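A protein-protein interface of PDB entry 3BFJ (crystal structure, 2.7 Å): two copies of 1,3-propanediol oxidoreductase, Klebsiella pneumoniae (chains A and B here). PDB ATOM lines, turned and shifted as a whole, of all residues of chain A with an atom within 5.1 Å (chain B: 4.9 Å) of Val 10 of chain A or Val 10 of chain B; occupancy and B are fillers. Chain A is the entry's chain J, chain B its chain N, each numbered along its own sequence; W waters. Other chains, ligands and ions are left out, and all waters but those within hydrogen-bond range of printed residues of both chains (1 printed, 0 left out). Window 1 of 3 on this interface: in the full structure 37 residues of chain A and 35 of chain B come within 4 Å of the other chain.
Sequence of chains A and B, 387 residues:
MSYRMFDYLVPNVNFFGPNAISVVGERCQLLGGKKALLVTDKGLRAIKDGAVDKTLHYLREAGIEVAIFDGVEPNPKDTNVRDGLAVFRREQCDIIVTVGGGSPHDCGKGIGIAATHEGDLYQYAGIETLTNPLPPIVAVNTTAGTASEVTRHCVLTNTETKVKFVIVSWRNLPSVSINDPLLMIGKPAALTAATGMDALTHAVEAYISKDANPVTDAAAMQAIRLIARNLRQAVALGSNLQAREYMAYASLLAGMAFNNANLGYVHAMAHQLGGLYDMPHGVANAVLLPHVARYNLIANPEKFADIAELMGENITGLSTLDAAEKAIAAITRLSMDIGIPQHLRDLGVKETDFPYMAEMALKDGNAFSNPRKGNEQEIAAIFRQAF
N of Val 10 of chain A sits at hydrogen-bond distance from O of Asn 12 of chain B, 3.2 Å away. The backbone NH of Tyr 8 of chain A is in hydrogen-bond range of the backbone carbonyl oxygen of Asn 14 of chain B, 2.6 Å away. The backbone carbonyl oxygen (O) of Asn 14 of chain A is in hydrogen-bond range of the backbone NH (N) of Tyr 8 of chain B. O of Asn 12 of chain A sits at hydrogen-bond distance from N of Val 10 of chain B, 3.2 Å away.
O of Leu 9 of chain B lies close to OD1 of Asn 259 of chain B (3.0 Å). O of Pro 11 of chain B sits close to OD1 of Asn 14 of chain B (2.8 Å). OD1 of Asn 259 of chain A lies close to O of Leu 9 of chain A, 3.2 Å away. The backbone carbonyl oxygen of Pro 11 of chain A lies close to the side-chain amide oxygen of Asn 14 of chain A, 3.0 Å away.
OH of Tyr 8 of chain A touches CE of Met 256 of chain B (3.97 Å). Asn 12 of chain B touches Leu 9 of chain A (O to CA, 3.5 Å). Val 10 of chain A touches Val 10 of chain B (CG1 to CG1, 3.3 Å). CG1 of Val 10 of chain B touches O of Pro 11 of chain A (3.7 Å). Pro 11 of chain A touches Asn 12 of chain B. O of Asn 12 of chain A touches CA of Leu 9 of chain B (3.5 Å). N of Asn 12 of chain A touches OD1 of Asn 12 of chain B, at 3.6 Å. CD2 of Leu 173 of chain B touches OD1 of Asn 12 of chain A, at 3.5 Å. Asn 12 of chain B touches Leu 173 of chain A (OD1 to CD2, 3.5 Å). CE of Met 256 of chain A touches OH of Tyr 8 of chain B, 3.6 Å away.
Of the printed residues of chain B, Val 10 of chain A touches Val 10 (3.3 Å) and Asn 12 (3.1 Å). Of chain A, only Val 10, Pro 11 and Asn 12 come within 4 Å of Val 10 of chain B. Of the printed residues of chain A, Asn 14 of chain B touches Tyr 8. Of the printed residues of chain B, Pro 11 of chain A touches Val 10 (3.7 Å) and Asn 12 (3.99 Å). The nearest printed residue of chain B that does not touch Val 10 of chain A is Pro 11 of chain B (4.02 Å). The nearest residue of chain A that does not touch Val 10 of chain B is Asn 14 of chain A (4.3 Å).
Of the 10 printed residues of chain A, 8 touch a printed residue of chain B.
Tyr 8 of chain A touches Asn 14 of chain B, and with the chains exchanged Asn 14 of chain A touches Tyr 8 of chain B. Val 10 of chain A touches its own counterpart, Val 10 of chain B. Val 10 of chain A touches Asn 12 of chain B, and with the chains exchanged Asn 12 of chain A touches Val 10 of chain B. Asn 12 of chain A touches its own counterpart, Asn 12 of chain B. Positions printed for both chains: 8, 9, 10, 11, 12, 14, 150, 173, 256 and 259. Of the 14 pairs that touch across the chains among the printed residues, 12 have their exchanged pair printed and touching as well.
Water W1 lies within hydrogen-bond range of the side-chain hydroxyl (OH) of Tyr 8 of chain A, the side-chain hydroxyl (OH) of Tyr 8 of chain B and the side-chain sulfur (SD) of Met 256 of chain B.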
ATOM      1  N   TYR A   8     -18.999 -29.346   9.453  1.00  0.00           N
ATOM      2  CA  TYR A   8     -19.238 -29.666   8.054  1.00  0.00           C
ATOM      3  C   TYR A   8     -20.334 -28.733   7.527  1.00  0.00           C
ATOM      4  O   TYR A   8     -21.518 -28.888   7.852  1.00  0.00           O
ATOM      5  CB  TYR A   8     -19.628 -31.141   7.922  1.00  0.00           C
ATOM      6  CG  TYR A   8     -19.749 -31.677   6.512  1.00  0.00           C
ATOM      7  CD1 TYR A   8     -18.628 -32.144   5.822  1.00  0.00           C
ATOM      8  CD2 TYR A   8     -20.990 -31.753   5.881  1.00  0.00           C
ATOM      9  CE1 TYR A   8     -18.734 -32.651   4.531  1.00  0.00           C
ATOM     10  CE2 TYR A   8     -21.107 -32.258   4.587  1.00  0.00           C
ATOM     11  CZ  TYR A   8     -19.975 -32.710   3.921  1.00  0.00           C
ATOM     12  OH  TYR A   8     -20.088 -33.217   2.647  1.00  0.00           O
ATOM     13  N   LEU A   9     -19.913 -27.744   6.741  1.00  0.00           N
ATOM     14  CA  LEU A   9     -20.807 -26.722   6.212  1.00  0.00           C
ATOM     15  C   LEU A   9     -21.065 -26.961   4.740  1.00  0.00           C
ATOM     16  O   LEU A   9     -20.177 -27.411   4.002  1.00  0.00           O
ATOM     17  CB  LEU A   9     -20.230 -25.317   6.400  1.00  0.00           C
ATOM     18  CG  LEU A   9     -19.591 -24.863   7.716  1.00  0.00           C
ATOM     19  CD1 LEU A   9     -19.316 -23.372   7.641  1.00  0.00           C
ATOM     20  CD2 LEU A   9     -20.428 -25.194   8.945  1.00  0.00           C
ATOM     21  N   VAL A  10     -22.292 -26.652   4.326  1.00  0.00           N
ATOM     22  CA  VAL A  10     -22.757 -26.868   2.960  1.00  0.00           C
ATOM     23  C   VAL A  10     -24.098 -26.147   2.816  1.00  0.00           C
ATOM     24  O   VAL A  10     -24.905 -26.165   3.753  1.00  0.00           O
ATOM     25  CB  VAL A  10     -22.868 -28.394   2.630  1.00  0.00           C
ATOM     26  CG1 VAL A  10     -23.649 -29.128   3.705  1.00  0.00           C
ATOM     27  CG2 VAL A  10     -23.460 -28.646   1.253  1.00  0.00           C
ATOM     28  N   PRO A  11     -24.327 -25.475   1.667  1.00  0.00           N
ATOM     29  CA  PRO A  11     -25.614 -24.826   1.414  1.00  0.00           C
ATOM     30  C   PRO A  11     -26.817 -25.715   1.727  1.00  0.00           C
ATOM     31  O   PRO A  11     -26.781 -26.926   1.510  1.00  0.00           O
ATOM     32  CB  PRO A  11     -25.561 -24.518  -0.082  1.00  0.00           C
ATOM     33  CG  PRO A  11     -24.127 -24.333  -0.373  1.00  0.00           C
ATOM     34  CD  PRO A  11     -23.381 -25.260   0.552  1.00  0.00           C
ATOM     35  N   ASN A  12     -27.860 -25.080   2.250  1.00  0.00           N
ATOM     36  CA  ASN A  12     -29.124 -25.708   2.630  1.00  0.00           C
ATOM     37  C   ASN A  12     -29.701 -26.604   1.535  1.00  0.00           C
ATOM     38  O   ASN A  12     -30.023 -27.774   1.764  1.00  0.00           O
ATOM     39  CB  ASN A  12     -30.132 -24.596   2.951  1.00  0.00           C
ATOM     40  CG  ASN A  12     -31.039 -24.935   4.110  1.00  0.00           C
ATOM     41  OD1 ASN A  12     -30.882 -25.967   4.762  1.00  0.00           O
ATOM     42  ND2 ASN A  12     -31.995 -24.052   4.384  1.00  0.00           N
ATOM     43  N   ASN A  14     -29.344 -27.758  -2.628  1.00  0.00           N
ATOM     44  CA  ASN A  14     -28.470 -27.831  -3.795  1.00  0.00           C
ATOM     45  C   ASN A  14     -29.152 -28.519  -4.972  1.00  0.00           C
ATOM     46  O   ASN A  14     -29.904 -29.475  -4.785  1.00  0.00           O
ATOM     47  CB  ASN A  14     -27.156 -28.540  -3.452  1.00  0.00           C
ATOM     48  CG  ASN A  14     -26.502 -27.993  -2.191  1.00  0.00           C
ATOM     49  OD1 ASN A  14     -26.865 -28.367  -1.074  1.00  0.00           O
ATOM     50  ND2 ASN A  14     -25.522 -27.120  -2.368  1.00  0.00           N
ATOM     51  N   VAL A 150     -20.559 -23.491  -3.153  1.00  0.00           N
ATOM     52  CA  VAL A 150     -20.797 -24.430  -2.064  1.00  0.00           C
ATOM     53  C   VAL A 150     -19.926 -24.101  -0.848  1.00  0.00           C
ATOM     54  O   VAL A 150     -19.997 -24.766   0.187  1.00  0.00           O
ATOM     55  CB  VAL A 150     -20.614 -25.895  -2.579  1.00  0.00           C
ATOM     56  CG1 VAL A 150     -19.553 -26.686  -1.789  1.00  0.00           C
ATOM     57  CG2 VAL A 150     -21.962 -26.616  -2.642  1.00  0.00           C
ATOM     58  N   LEU A 173     -22.087 -19.114   3.069  1.00  0.00           N
ATOM     59  CA  LEU A 173     -22.711 -20.254   2.407  1.00  0.00           C
ATOM     60  C   LEU A 173     -23.945 -19.789   1.642  1.00  0.00           C
ATOM     61  O   LEU A 173     -24.895 -19.274   2.252  1.00  0.00           O
ATOM     62  CB  LEU A 173     -23.108 -21.311   3.437  1.00  0.00           C
ATOM     63  CG  LEU A 173     -22.376 -22.651   3.553  1.00  0.00           C
ATOM     64  CD1 LEU A 173     -20.873 -22.525   3.498  1.00  0.00           C
ATOM     65  CD2 LEU A 173     -22.801 -23.319   4.845  1.00  0.00           C
ATOM     66  N   MET A 256     -17.500 -29.831  -1.404  1.00  0.00           N
ATOM     67  CA  MET A 256     -18.051 -30.286  -0.132  1.00  0.00           C
ATOM     68  C   MET A 256     -16.940 -30.810   0.779  1.00  0.00           C
ATOM     69  O   MET A 256     -16.996 -30.659   2.006  1.00  0.00           O
ATOM     70  CB  MET A 256     -19.113 -31.363  -0.361  1.00  0.00           C
ATOM     71  CG  MET A 256     -20.434 -30.825  -0.902  1.00  0.00           C
ATOM     72  SD  MET A 256     -21.478 -32.102  -1.649  1.00  0.00           S
ATOM     73  CE  MET A 256     -21.952 -33.056  -0.214  1.00  0.00           C
ATOM     74  N   ASN A 259     -14.130 -27.652   1.525  1.00  0.00           N
ATOM     75  CA  ASN A 259     -14.757 -26.618   2.338  1.00  0.00           C
ATOM     76  C   ASN A 259     -14.650 -26.946   3.822  1.00  0.00           C
ATOM     77  O   ASN A 259     -14.638 -26.049   4.662  1.00  0.00           O
ATOM     78  CB  ASN A 259     -16.223 -26.420   1.945  1.00  0.00           C
ATOM     79  CG  ASN A 259     -16.860 -25.219   2.629  1.00  0.00           C
ATOM     80  OD1 ASN A 259     -17.919 -25.329   3.255  1.00  0.00           O
ATOM     81  ND2 ASN A 259     -16.215 -24.069   2.512  1.00  0.00           N
ATOM     82  N   TYR B   8     -30.431 -31.775  -3.538  1.00  0.00           N
ATOM     83  CA  TYR B   8     -29.586 -32.292  -2.469  1.00  0.00           C
ATOM     84  C   TYR B   8     -29.695 -31.378  -1.261  1.00  0.00           C
ATOM     85  O   TYR B   8     -29.128 -30.283  -1.237  1.00  0.00           O
ATOM     86  CB  TYR B   8     -28.130 -32.408  -2.938  1.00  0.00           C
ATOM     87  CG  TYR B   8     -27.217 -33.174  -2.000  1.00  0.00           C
ATOM     88  CD1 TYR B   8     -27.032 -34.549  -2.143  1.00  0.00           C
ATOM     89  CD2 TYR B   8     -26.529 -32.521  -0.977  1.00  0.00           C
ATOM     90  CE1 TYR B   8     -26.189 -35.260  -1.280  1.00  0.00           C
ATOM     91  CE2 TYR B   8     -25.687 -33.221  -0.115  1.00  0.00           C
ATOM     92  CZ  TYR B   8     -25.520 -34.588  -0.274  1.00  0.00           C
ATOM     93  OH  TYR B   8     -24.690 -35.272   0.578  1.00  0.00           O
ATOM     94  N   LEU B   9     -30.446 -31.839  -0.267  1.00  0.00           N
ATOM     95  CA  LEU B   9     -30.689 -31.068   0.947  1.00  0.00           C
ATOM     96  C   LEU B   9     -29.909 -31.641   2.118  1.00  0.00           C
ATOM     97  O   LEU B   9     -29.778 -32.862   2.269  1.00  0.00           O
ATOM     98  CB  LEU B   9     -32.181 -31.005   1.299  1.00  0.00           C
ATOM     99  CG  LEU B   9     -33.306 -30.837   0.266  1.00  0.00           C
ATOM    100  CD1 LEU B   9     -34.572 -30.407   0.992  1.00  0.00           C
ATOM    101  CD2 LEU B   9     -32.982 -29.861  -0.865  1.00  0.00           C
ATOM    102  N   VAL B  10     -29.400 -30.734   2.943  1.00  0.00           N
ATOM    103  CA  VAL B  10     -28.594 -31.076   4.106  1.00  0.00           C
ATOM    104  C   VAL B  10     -28.653 -29.871   5.046  1.00  0.00           C
ATOM    105  O   VAL B  10     -28.741 -28.731   4.574  1.00  0.00           O
ATOM    106  CB  VAL B  10     -27.133 -31.445   3.682  1.00  0.00           C
ATOM    107  CG1 VAL B  10     -26.544 -30.384   2.762  1.00  0.00           C
ATOM    108  CG2 VAL B  10     -26.232 -31.695   4.885  1.00  0.00           C
ATOM    109  N   PRO B  11     -28.674 -30.108   6.374  1.00  0.00           N
ATOM    110  CA  PRO B  11     -28.569 -28.973   7.294  1.00  0.00           C
ATOM    111  C   PRO B  11     -27.368 -28.094   6.974  1.00  0.00           C
ATOM    112  O   PRO B  11     -26.292 -28.598   6.684  1.00  0.00           O
ATOM    113  CB  PRO B  11     -28.397 -29.641   8.655  1.00  0.00           C
ATOM    114  CG  PRO B  11     -29.117 -30.932   8.512  1.00  0.00           C
ATOM    115  CD  PRO B  11     -28.846 -31.382   7.098  1.00  0.00           C
ATOM    116  N   ASN B  12     -27.587 -26.788   7.000  1.00  0.00           N
ATOM    117  CA  ASN B  12     -26.571 -25.771   6.735  1.00  0.00           C
ATOM    118  C   ASN B  12     -25.230 -26.043   7.423  1.00  0.00           C
ATOM    119  O   ASN B  12     -24.179 -26.049   6.784  1.00  0.00           O
ATOM    120  CB  ASN B  12     -27.115 -24.409   7.198  1.00  0.00           C
ATOM    121  CG  ASN B  12     -26.796 -23.286   6.237  1.00  0.00           C
ATOM    122  OD1 ASN B  12     -26.325 -23.513   5.119  1.00  0.00           O
ATOM    123  ND2 ASN B  12     -27.066 -22.060   6.662  1.00  0.00           N
ATOM    124  N   ASN B  14     -23.134 -28.494  10.329  1.00  0.00           N
ATOM    125  CA  ASN B  14     -23.105 -29.781  11.035  1.00  0.00           C
ATOM    126  C   ASN B  14     -21.846 -29.977  11.855  1.00  0.00           C
ATOM    127  O   ASN B  14     -20.746 -29.640  11.406  1.00  0.00           O
ATOM    128  CB  ASN B  14     -23.254 -30.955  10.062  1.00  0.00           C
ATOM    129  CG  ASN B  14     -24.438 -30.800   9.146  1.00  0.00           C
ATOM    130  OD1 ASN B  14     -24.379 -30.074   8.155  1.00  0.00           O
ATOM    131  ND2 ASN B  14     -25.525 -31.481   9.468  1.00  0.00           N
ATOM    132  N   VAL B 150     -30.775 -34.835  10.091  1.00  0.00           N
ATOM    133  CA  VAL B 150     -30.234 -34.466   8.787  1.00  0.00           C
ATOM    134  C   VAL B 150     -31.339 -34.522   7.725  1.00  0.00           C
ATOM    135  O   VAL B 150     -31.154 -34.109   6.576  1.00  0.00           O
ATOM    136  CB  VAL B 150     -28.978 -35.344   8.465  1.00  0.00           C
ATOM    137  CG1 VAL B 150     -28.932 -35.836   7.014  1.00  0.00           C
ATOM    138  CG2 VAL B 150     -27.719 -34.585   8.838  1.00  0.00           C
ATOM    139  N   LEU B 173     -35.551 -29.213   7.583  1.00  0.00           N
ATOM    140  CA  LEU B 173     -34.115 -29.318   7.814  1.00  0.00           C
ATOM    141  C   LEU B 173     -33.679 -28.515   9.025  1.00  0.00           C
ATOM    142  O   LEU B 173     -33.792 -27.289   9.020  1.00  0.00           O
ATOM    143  CB  LEU B 173     -33.370 -28.793   6.589  1.00  0.00           C
ATOM    144  CG  LEU B 173     -32.615 -29.707   5.624  1.00  0.00           C
ATOM    145  CD1 LEU B 173     -33.214 -31.104   5.504  1.00  0.00           C
ATOM    146  CD2 LEU B 173     -32.545 -29.021   4.269  1.00  0.00           C
ATOM    147  N   MET B 256     -27.344 -38.487   4.713  1.00  0.00           N
ATOM    148  CA  MET B 256     -27.102 -37.552   3.617  1.00  0.00           C
ATOM    149  C   MET B 256     -27.444 -38.212   2.282  1.00  0.00           C
ATOM    150  O   MET B 256     -27.791 -37.529   1.306  1.00  0.00           O
ATOM    151  CB  MET B 256     -25.652 -37.054   3.642  1.00  0.00           C
ATOM    152  CG  MET B 256     -25.397 -35.946   4.666  1.00  0.00           C
ATOM    153  SD  MET B 256     -23.696 -35.740   5.269  1.00  0.00           S
ATOM    154  CE  MET B 256     -22.737 -35.946   3.774  1.00  0.00           C
ATOM    155  N   ASN B 259     -31.712 -39.204   2.403  1.00  0.00           N
ATOM    156  CA  ASN B 259     -32.489 -37.974   2.470  1.00  0.00           C
ATOM    157  C   ASN B 259     -32.717 -37.424   1.071  1.00  0.00           C
ATOM    158  O   ASN B 259     -33.685 -36.702   0.824  1.00  0.00           O
ATOM    159  CB  ASN B 259     -31.783 -36.932   3.339  1.00  0.00           C
ATOM    160  CG  ASN B 259     -32.576 -35.645   3.481  1.00  0.00           C
ATOM    161  OD1 ASN B 259     -32.092 -34.570   3.134  1.00  0.00           O
ATOM    162  ND2 ASN B 259     -33.801 -35.749   3.989  1.00  0.00           N
HETATM  163  O   HOH W   1     -22.974 -33.540   2.411  1.00  0.00           O
